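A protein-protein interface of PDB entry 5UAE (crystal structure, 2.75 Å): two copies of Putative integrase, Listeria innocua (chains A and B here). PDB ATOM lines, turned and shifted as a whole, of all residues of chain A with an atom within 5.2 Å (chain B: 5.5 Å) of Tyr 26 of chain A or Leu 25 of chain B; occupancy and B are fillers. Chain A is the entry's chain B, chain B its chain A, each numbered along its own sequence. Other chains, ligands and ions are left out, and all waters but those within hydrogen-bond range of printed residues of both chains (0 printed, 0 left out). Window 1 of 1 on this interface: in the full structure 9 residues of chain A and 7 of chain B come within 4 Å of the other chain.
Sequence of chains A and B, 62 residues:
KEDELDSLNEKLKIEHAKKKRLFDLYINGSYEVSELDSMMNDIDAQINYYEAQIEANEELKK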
ATOM      1  N   LEU A  22      12.406 -30.453 -19.897  1.00  0.00           N
ATOM      2  CA  LEU A  22      12.037 -29.088 -19.542  1.00  0.00           C
ATOM      3  C   LEU A  22      12.565 -28.730 -18.158  1.00  0.00           C
ATOM      4  O   LEU A  22      13.043 -27.617 -17.933  1.00  0.00           O
ATOM      5  CB  LEU A  22      10.520 -28.911 -19.590  1.00  0.00           C
ATOM      6  CG  LEU A  22      10.019 -27.466 -19.551  1.00  0.00           C
ATOM      7  CD1 LEU A  22      10.489 -26.718 -20.782  1.00  0.00           C
ATOM      8  CD2 LEU A  22       8.511 -27.420 -19.456  1.00  0.00           C
ATOM      9  N   PHE A  23      12.469 -29.684 -17.237  1.00  0.00           N
ATOM     10  CA  PHE A  23      13.008 -29.524 -15.894  1.00  0.00           C
ATOM     11  C   PHE A  23      14.510 -29.251 -15.941  1.00  0.00           C
ATOM     12  O   PHE A  23      15.007 -28.346 -15.275  1.00  0.00           O
ATOM     13  CB  PHE A  23      12.716 -30.771 -15.057  1.00  0.00           C
ATOM     14  CG  PHE A  23      11.372 -30.752 -14.380  1.00  0.00           C
ATOM     15  CD1 PHE A  23      10.975 -29.659 -13.628  1.00  0.00           C
ATOM     16  CD2 PHE A  23      10.508 -31.831 -14.492  1.00  0.00           C
ATOM     17  CE1 PHE A  23       9.742 -29.642 -12.999  1.00  0.00           C
ATOM     18  CE2 PHE A  23       9.274 -31.820 -13.866  1.00  0.00           C
ATOM     19  CZ  PHE A  23       8.890 -30.724 -13.119  1.00  0.00           C
ATOM     20  N   ASP A  24      15.217 -30.037 -16.749  1.00  0.00           N
ATOM     21  CA  ASP A  24      16.659 -29.895 -16.933  1.00  0.00           C
ATOM     22  C   ASP A  24      17.019 -28.495 -17.427  1.00  0.00           C
ATOM     23  O   ASP A  24      17.966 -27.878 -16.937  1.00  0.00           O
ATOM     24  CB  ASP A  24      17.159 -30.956 -17.921  1.00  0.00           C
ATOM     25  CG  ASP A  24      18.671 -31.112 -17.916  1.00  0.00           C
ATOM     26  OD1 ASP A  24      19.371 -30.284 -17.297  1.00  0.00           O
ATOM     27  OD2 ASP A  24      19.160 -32.072 -18.547  1.00  0.00           O
ATOM     28  N   LEU A  25      16.249 -28.004 -18.392  1.00  0.00           N
ATOM     29  CA  LEU A  25      16.500 -26.704 -19.003  1.00  0.00           C
ATOM     30  C   LEU A  25      16.365 -25.544 -18.018  1.00  0.00           C
ATOM     31  O   LEU A  25      17.241 -24.680 -17.951  1.00  0.00           O
ATOM     32  CB  LEU A  25      15.557 -26.495 -20.189  1.00  0.00           C
ATOM     33  CG  LEU A  25      15.813 -27.400 -21.398  1.00  0.00           C
ATOM     34  CD1 LEU A  25      14.826 -27.121 -22.517  1.00  0.00           C
ATOM     35  CD2 LEU A  25      17.241 -27.233 -21.892  1.00  0.00           C
ATOM     36  N   TYR A  26      15.271 -25.523 -17.261  1.00  0.00           N
ATOM     37  CA  TYR A  26      15.044 -24.453 -16.291  1.00  0.00           C
ATOM     38  C   TYR A  26      16.139 -24.408 -15.240  1.00  0.00           C
ATOM     39  O   TYR A  26      16.647 -23.333 -14.906  1.00  0.00           O
ATOM     40  CB  TYR A  26      13.695 -24.612 -15.594  1.00  0.00           C
ATOM     41  CG  TYR A  26      13.550 -23.712 -14.385  1.00  0.00           C
ATOM     42  CD1 TYR A  26      13.209 -22.377 -14.533  1.00  0.00           C
ATOM     43  CD2 TYR A  26      13.774 -24.192 -13.099  1.00  0.00           C
ATOM     44  CE1 TYR A  26      13.087 -21.545 -13.438  1.00  0.00           C
ATOM     45  CE2 TYR A  26      13.659 -23.367 -11.999  1.00  0.00           C
ATOM     46  CZ  TYR A  26      13.313 -22.045 -12.173  1.00  0.00           C
ATOM     47  OH  TYR A  26      13.191 -21.220 -11.079  1.00  0.00           O
ATOM     48  N   ILE A  27      16.476 -25.583 -14.714  1.00  0.00           N
ATOM     49  CA  ILE A  27      17.502 -25.729 -13.686  1.00  0.00           C
ATOM     50  C   ILE A  27      18.821 -25.113 -14.139  1.00  0.00           C
ATOM     51  O   ILE A  27      19.552 -24.521 -13.341  1.00  0.00           O
ATOM     52  CB  ILE A  27      17.712 -27.217 -13.323  1.00  0.00           C
ATOM     53  CG1 ILE A  27      16.464 -27.768 -12.628  1.00  0.00           C
ATOM     54  CG2 ILE A  27      18.925 -27.401 -12.437  1.00  0.00           C
ATOM     55  CD1 ILE A  27      16.519 -29.245 -12.335  1.00  0.00           C
ATOM     56  N   ASN A  28      19.102 -25.227 -15.434  1.00  0.00           N
ATOM     57  CA  ASN A  28      20.301 -24.635 -16.017  1.00  0.00           C
ATOM     58  C   ASN A  28      20.092 -23.170 -16.398  1.00  0.00           C
ATOM     59  O   ASN A  28      20.896 -22.585 -17.123  1.00  0.00           O
ATOM     60  CB  ASN A  28      20.750 -25.431 -17.244  1.00  0.00           C
ATOM     61  CG  ASN A  28      21.222 -26.829 -16.893  1.00  0.00           C
ATOM     62  OD1 ASN A  28      22.419 -27.076 -16.740  1.00  0.00           O
ATOM     63  ND2 ASN A  28      20.280 -27.755 -16.765  1.00  0.00           N
ATOM     64  N   GLY A  29      18.998 -22.587 -15.916  1.00  0.00           N
ATOM     65  CA  GLY A  29      18.738 -21.170 -16.096  1.00  0.00           C
ATOM     66  C   GLY A  29      18.350 -20.746 -17.501  1.00  0.00           C
ATOM     67  O   GLY A  29      18.615 -19.615 -17.903  1.00  0.00           O
ATOM     68  N   SER A  30      17.713 -21.640 -18.247  1.00  0.00           N
ATOM     69  CA  SER A  30      17.318 -21.332 -19.618  1.00  0.00           C
ATOM     70  C   SER A  30      15.958 -20.637 -19.687  1.00  0.00           C
ATOM     71  O   SER A  30      15.710 -19.832 -20.586  1.00  0.00           O
ATOM     72  CB  SER A  30      17.294 -22.605 -20.465  1.00  0.00           C
ATOM     73  OG  SER A  30      18.579 -23.203 -20.519  1.00  0.00           O
ATOM     74  N   TYR A  31      15.078 -20.951 -18.741  1.00  0.00           N
ATOM     75  CA  TYR A  31      13.731 -20.387 -18.741  1.00  0.00           C
ATOM     76  C   TYR A  31      13.404 -19.668 -17.434  1.00  0.00           C
ATOM     77  O   TYR A  31      13.992 -19.949 -16.389  1.00  0.00           O
ATOM     78  CB  TYR A  31      12.690 -21.482 -18.998  1.00  0.00           C
ATOM     79  CG  TYR A  31      12.618 -21.955 -20.439  1.00  0.00           C
ATOM     80  CD1 TYR A  31      11.769 -21.340 -21.351  1.00  0.00           C
ATOM     81  CD2 TYR A  31      13.394 -23.018 -20.883  1.00  0.00           C
ATOM     82  CE1 TYR A  31      11.697 -21.769 -22.667  1.00  0.00           C
ATOM     83  CE2 TYR A  31      13.329 -23.454 -22.198  1.00  0.00           C
ATOM     84  CZ  TYR A  31      12.479 -22.825 -23.086  1.00  0.00           C
ATOM     85  OH  TYR A  31      12.406 -23.248 -24.394  1.00  0.00           O
ATOM     86  N   GLU A  32      12.465 -18.728 -17.508  1.00  0.00           N
ATOM     87  CA  GLU A  32      11.940 -18.050 -16.327  1.00  0.00           C
ATOM     88  C   GLU A  32      10.752 -18.829 -15.771  1.00  0.00           C
ATOM     89  O   GLU A  32      10.013 -19.465 -16.524  1.00  0.00           O
ATOM     90  CB  GLU A  32      11.537 -16.605 -16.661  1.00  0.00           C
ATOM     91  CG  GLU A  32      10.691 -15.914 -15.592  1.00  0.00           C
ATOM     92  CD  GLU A  32      10.785 -14.401 -15.637  1.00  0.00           C
ATOM     93  OE1 GLU A  32      11.615 -13.883 -16.408  1.00  0.00           O
ATOM     94  OE2 GLU A  32      10.030 -13.733 -14.896  1.00  0.00           O
ATOM     95  N   VAL A  33      10.599 -18.778 -14.449  1.00  0.00           N
ATOM     96  CA  VAL A  33       9.530 -19.457 -13.718  1.00  0.00           C
ATOM     97  C   VAL A  33       8.143 -19.363 -14.368  1.00  0.00           C
ATOM     98  O   VAL A  33       7.482 -20.385 -14.568  1.00  0.00           O
ATOM     99  CB  VAL A  33       9.420 -18.904 -12.283  1.00  0.00           C
ATOM    100  CG1 VAL A  33       8.513 -19.785 -11.457  1.00  0.00           C
ATOM    101  CG2 VAL A  33      10.803 -18.800 -11.639  1.00  0.00           C
ATOM    102  N   LEU A  36       7.660 -21.468 -17.453  1.00  0.00           N
ATOM    103  CA  LEU A  36       7.703 -22.890 -17.137  1.00  0.00           C
ATOM    104  C   LEU A  36       6.333 -23.453 -16.779  1.00  0.00           C
ATOM    105  O   LEU A  36       5.938 -24.507 -17.280  1.00  0.00           O
ATOM    106  CB  LEU A  36       8.680 -23.143 -15.986  1.00  0.00           C
ATOM    107  CG  LEU A  36       8.855 -24.602 -15.560  1.00  0.00           C
ATOM    108  CD1 LEU A  36       9.785 -25.333 -16.514  1.00  0.00           C
ATOM    109  CD2 LEU A  36       9.356 -24.689 -14.130  1.00  0.00           C
ATOM    110  N   ARG B  21      17.885 -22.480  -8.250  1.00  0.00           N
ATOM    111  CA  ARG B  21      16.840 -22.529  -9.263  1.00  0.00           C
ATOM    112  C   ARG B  21      15.793 -23.573  -8.894  1.00  0.00           C
ATOM    113  O   ARG B  21      14.595 -23.343  -9.053  1.00  0.00           O
ATOM    114  CB  ARG B  21      17.432 -22.832 -10.640  1.00  0.00           C
ATOM    115  CG  ARG B  21      18.308 -21.721 -11.199  1.00  0.00           C
ATOM    116  CD  ARG B  21      17.482 -20.552 -11.715  1.00  0.00           C
ATOM    117  NE  ARG B  21      16.888 -20.836 -13.018  1.00  0.00           N
ATOM    118  CZ  ARG B  21      16.217 -19.947 -13.745  1.00  0.00           C
ATOM    119  NH1 ARG B  21      16.048 -18.711 -13.298  1.00  0.00           N
ATOM    120  NH2 ARG B  21      15.713 -20.295 -14.920  1.00  0.00           N
ATOM    121  N   LEU B  22      16.256 -24.716  -8.396  1.00  0.00           N
ATOM    122  CA  LEU B  22      15.364 -25.789  -7.977  1.00  0.00           C
ATOM    123  C   LEU B  22      14.535 -25.393  -6.758  1.00  0.00           C
ATOM    124  O   LEU B  22      13.373 -25.782  -6.639  1.00  0.00           O
ATOM    125  CB  LEU B  22      16.162 -27.060  -7.675  1.00  0.00           C
ATOM    126  CG  LEU B  22      15.361 -28.289  -7.232  1.00  0.00           C
ATOM    127  CD1 LEU B  22      14.250 -28.603  -8.223  1.00  0.00           C
ATOM    128  CD2 LEU B  22      16.273 -29.492  -7.056  1.00  0.00           C
ATOM    129  N   PHE B  23      15.134 -24.624  -5.853  1.00  0.00           N
ATOM    130  CA  PHE B  23      14.429 -24.184  -4.656  1.00  0.00           C
ATOM    131  C   PHE B  23      13.289 -23.237  -5.005  1.00  0.00           C
ATOM    132  O   PHE B  23      12.296 -23.159  -4.282  1.00  0.00           O
ATOM    133  CB  PHE B  23      15.391 -23.516  -3.678  1.00  0.00           C
ATOM    134  CG  PHE B  23      16.016 -24.469  -2.706  1.00  0.00           C
ATOM    135  CD1 PHE B  23      15.243 -25.093  -1.743  1.00  0.00           C
ATOM    136  CD2 PHE B  23      17.372 -24.738  -2.746  1.00  0.00           C
ATOM    137  CE1 PHE B  23      15.808 -25.970  -0.843  1.00  0.00           C
ATOM    138  CE2 PHE B  23      17.943 -25.615  -1.850  1.00  0.00           C
ATOM    139  CZ  PHE B  23      17.162 -26.232  -0.898  1.00  0.00           C
ATOM    140  N   ASP B  24      13.440 -22.522  -6.116  1.00  0.00           N
ATOM    141  CA  ASP B  24      12.374 -21.670  -6.624  1.00  0.00           C
ATOM    142  C   ASP B  24      11.134 -22.503  -6.931  1.00  0.00           C
ATOM    143  O   ASP B  24      10.008 -22.070  -6.693  1.00  0.00           O
ATOM    144  CB  ASP B  24      12.836 -20.915  -7.870  1.00  0.00           C
ATOM    145  CG  ASP B  24      13.868 -19.848  -7.558  1.00  0.00           C
ATOM    146  OD1 ASP B  24      13.890 -19.358  -6.409  1.00  0.00           O
ATOM    147  OD2 ASP B  24      14.651 -19.494  -8.463  1.00  0.00           O
ATOM    148  N   LEU B  25      11.357 -23.707  -7.450  1.00  0.00           N
ATOM    149  CA  LEU B  25      10.276 -24.635  -7.765  1.00  0.00           C
ATOM    150  C   LEU B  25       9.600 -25.158  -6.502  1.00  0.00           C
ATOM    151  O   LEU B  25       8.375 -25.266  -6.441  1.00  0.00           O
ATOM    152  CB  LEU B  25      10.806 -25.803  -8.598  1.00  0.00           C
ATOM    153  CG  LEU B  25      11.496 -25.394  -9.903  1.00  0.00           C
ATOM    154  CD1 LEU B  25      11.896 -26.610 -10.719  1.00  0.00           C
ATOM    155  CD2 LEU B  25      10.589 -24.481 -10.708  1.00  0.00           C
ATOM    156  N   TYR B  26      10.412 -25.486  -5.503  1.00  0.00           N
ATOM    157  CA  TYR B  26       9.909 -25.943  -4.213  1.00  0.00           C
ATOM    158  C   TYR B  26       8.992 -24.904  -3.585  1.00  0.00           C
ATOM    159  O   TYR B  26       7.908 -25.230  -3.095  1.00  0.00           O
ATOM    160  CB  TYR B  26      11.066 -26.244  -3.264  1.00  0.00           C
ATOM    161  CG  TYR B  26      11.624 -27.645  -3.363  1.00  0.00           C
ATOM    162  CD1 TYR B  26      11.053 -28.688  -2.648  1.00  0.00           C
ATOM    163  CD2 TYR B  26      12.735 -27.919  -4.149  1.00  0.00           C
ATOM    164  CE1 TYR B  26      11.563 -29.967  -2.724  1.00  0.00           C
ATOM    165  CE2 TYR B  26      13.252 -29.197  -4.230  1.00  0.00           C
ATOM    166  CZ  TYR B  26      12.662 -30.216  -3.516  1.00  0.00           C
ATOM    167  OH  TYR B  26      13.175 -31.488  -3.594  1.00  0.00           O
ATOM    168  N   ILE B  27       9.446 -23.653  -3.610  1.00  0.00           N
ATOM    169  CA  ILE B  27       8.698 -22.524  -3.064  1.00  0.00           C
ATOM    170  C   ILE B  27       7.350 -22.374  -3.754  1.00  0.00           C
ATOM    171  O   ILE B  27       6.314 -22.275  -3.093  1.00  0.00           O
ATOM    172  CB  ILE B  27       9.493 -21.210  -3.203  1.00  0.00           C
ATOM    173  CG1 ILE B  27      10.758 -21.261  -2.346  1.00  0.00           C
ATOM    174  CG2 ILE B  27       8.642 -20.023  -2.808  1.00  0.00           C
ATOM    175  CD1 ILE B  27      11.625 -20.035  -2.458  1.00  0.00           C
ATOM    176  N   ASN B  28       7.371 -22.365  -5.084  1.00  0.00           N
ATOM    177  CA  ASN B  28       6.144 -22.305  -5.870  1.00  0.00           C
ATOM    178  C   ASN B  28       5.294 -23.548  -5.663  1.00  0.00           C
ATOM    179  O   ASN B  28       4.067 -23.488  -5.710  1.00  0.00           O
ATOM    180  CB  ASN B  28       6.463 -22.133  -7.358  1.00  0.00           C
ATOM    181  CG  ASN B  28       5.217 -22.130  -8.228  1.00  0.00           C
ATOM    182  OD1 ASN B  28       4.805 -23.169  -8.747  1.00  0.00           O
ATOM    183  ND2 ASN B  28       4.610 -20.961  -8.389  1.00  0.00           N
ATOM    184  N   GLY B  29       5.958 -24.675  -5.431  1.00  0.00           N
ATOM    185  CA  GLY B  29       5.268 -25.938  -5.253  1.00  0.00           C
ATOM    186  C   GLY B  29       4.502 -26.378  -6.486  1.00  0.00           C
ATOM    187  O   GLY B  29       4.784 -25.923  -7.593  1.00  0.00           O
ATOM    188  N   SER B  30       3.537 -27.275  -6.285  1.00  0.00           N
ATOM    189  CA  SER B  30       2.684 -27.829  -7.345  1.00  0.00           C
ATOM    190  C   SER B  30       3.451 -28.718  -8.329  1.00  0.00           C
ATOM    191  O   SER B  30       2.852 -29.356  -9.195  1.00  0.00           O
ATOM    192  CB  SER B  30       1.957 -26.718  -8.111  1.00  0.00           C
ATOM    193  OG  SER B  30       2.840 -25.983  -8.938  1.00  0.00           O
ATOM    194  N   TYR B  31       4.773 -28.761  -8.197  1.00  0.00           N
ATOM    195  CA  TYR B  31       5.576 -29.745  -8.907  1.00  0.00           C
ATOM    196  C   TYR B  31       5.890 -30.867  -7.930  1.00  0.00           C
ATOM    197  O   TYR B  31       6.473 -30.626  -6.873  1.00  0.00           O
ATOM    198  CB  TYR B  31       6.856 -29.120  -9.465  1.00  0.00           C
ATOM    199  CG  TYR B  31       6.617 -27.893 -10.321  1.00  0.00           C
ATOM    200  CD1 TYR B  31       6.325 -28.008 -11.674  1.00  0.00           C
ATOM    201  CD2 TYR B  31       6.680 -26.621  -9.772  1.00  0.00           C
ATOM    202  CE1 TYR B  31       6.101 -26.886 -12.454  1.00  0.00           C
ATOM    203  CE2 TYR B  31       6.456 -25.496 -10.541  1.00  0.00           C
ATOM    204  CZ  TYR B  31       6.169 -25.633 -11.881  1.00  0.00           C
ATOM    205  OH  TYR B  31       5.948 -24.512 -12.649  1.00  0.00           O
ATOM    206  N   LEU B  36      10.932 -33.334  -7.649  1.00  0.00           N
ATOM    207  CA  LEU B  36      11.880 -32.314  -7.220  1.00  0.00           C
ATOM    208  C   LEU B  36      12.986 -32.910  -6.355  1.00  0.00           C
ATOM    209  O   LEU B  36      14.146 -32.509  -6.454  1.00  0.00           O
ATOM    210  CB  LEU B  36      11.159 -31.201  -6.454  1.00  0.00           C
ATOM    211  CG  LEU B  36      10.107 -30.387  -7.216  1.00  0.00           C
ATOM    212  CD1 LEU B  36       9.566 -29.262  -6.348  1.00  0.00           C
ATOM    213  CD2 LEU B  36      10.680 -29.835  -8.512  1.00  0.00           C
ATOM    214  N   MET B  39      15.886 -34.625  -8.278  1.00  0.00           N
ATOM    215  CA  MET B  39      16.820 -33.627  -8.786  1.00  0.00           C
ATOM    216  C   MET B  39      17.684 -33.071  -7.661  1.00  0.00           C
ATOM    217  O   MET B  39      18.876 -32.824  -7.846  1.00  0.00           O
ATOM    218  CB  MET B  39      16.068 -32.490  -9.474  1.00  0.00           C
ATOM    219  CG  MET B  39      14.973 -32.966 -10.405  1.00  0.00           C
ATOM    220  SD  MET B  39      13.908 -31.636 -10.994  1.00  0.00           S
ATOM    221  CE  MET B  39      12.603 -32.592 -11.755  1.00  0.00           C
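Printed residues of chain A that touch a printed residue of chain B: Phe 23, Tyr 26, Ile 27, Gly 29, Tyr 31 and Leu 36.
Hydrophobic or aromatic side chains of chain A that line the printed part of chain B: Phe 23, Tyr 26, Ile 27 and Leu 36.
Of the 13 printed residues of chain B, 5 touch a printed residue of chain A.
Among the printed residues, 10 pairs touch across the chains.
Among the printed residues, no Asp or Glu carboxylate lies within 4 Å of a Lys or Arg side-chain nitrogen of the other chain.
Among the printed residues, pairs that only touch across the chains: Gly 29 of chain A with Arg 21 of chain B, Phe 23 of chain A with Met 39 of chain B, Tyr 26 of chain A with Leu 25 of chain B, Leu 36 of chain A with Leu 25 of chain B, Leu 36 of chain A with Tyr 31 of chain B, Ile 27 of chain A with Arg 21 of chain B and Ile 27 of chain A with Met 39 of chain B.
The guanidinium group (NE) of Arg 21 of chain B lies within hydrogen-bond range of the backbone carbonyl oxygen (O) of Tyr 26 of chain A, 3.1 Å away.
The side-chain carboxylate of Asp 24 of chain B sits close to the side-chain hydroxyl of Tyr 26 of chain A (3.5 Å).
O of Tyr 31 of chain A sits close to NH2 of Arg 21 of chain B, at 2.3 Å.
Tyr 26 of chain A touches Asp 24 of chain B, but with the chains exchanged Asp 24 of chain A does not touch Tyr 26 of chain B (12.7 Å).
Tyr 26 of chain A touches Leu 25 of chain B, but with the chains exchanged Leu 25 of chain A does not touch Tyr 26 of chain B (13.9 Å).
Leu 36 of chain A touches Leu 25 of chain B, but with the chains exchanged Leu 25 of chain A does not touch Leu 36 of chain B (11.5 Å).
Leu 36 of chain A touches Tyr 31 of chain B, but with the chains exchanged Tyr 31 of chain A does not touch Leu 36 of chain B (13.1 Å).
11 positions are printed for both chains.
Leu 22 of chain A touches none of the printed residues of chain B.
Tyr 26 of chain A touches just these residues of chain B: Arg 21, Asp 24 and Leu 25.
Of the printed residues of chain B, Ile 27 of chain A touches Arg 21 (3.7 Å) and Met 39 (3.8 Å).
Of the printed residues of chain B, Gly 29 of chain A touches Arg 21 (3.4 Å).
Of the printed residues of chain B, Leu 36 of chain A touches Leu 25 and Tyr 31.
Of the printed residues of chain A, Arg 21 of chain B touches Tyr 26, Ile 27, Gly 29 and Tyr 31.
Of chain A, only Tyr 26 (3.5 Å) and Leu 36 (3.6 Å) come within 4 Å of Leu 25 of chain B.
Ser 30 of chain B touches none of the printed residues of chain A.
Printed residues of chain A within 4 Å of Tyr 31 of chain B: Leu 36 (3.7 Å).
The nearest residue of chain A that does not touch Leu 25 of chain B is Phe 23 of chain A (4.3 Å).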
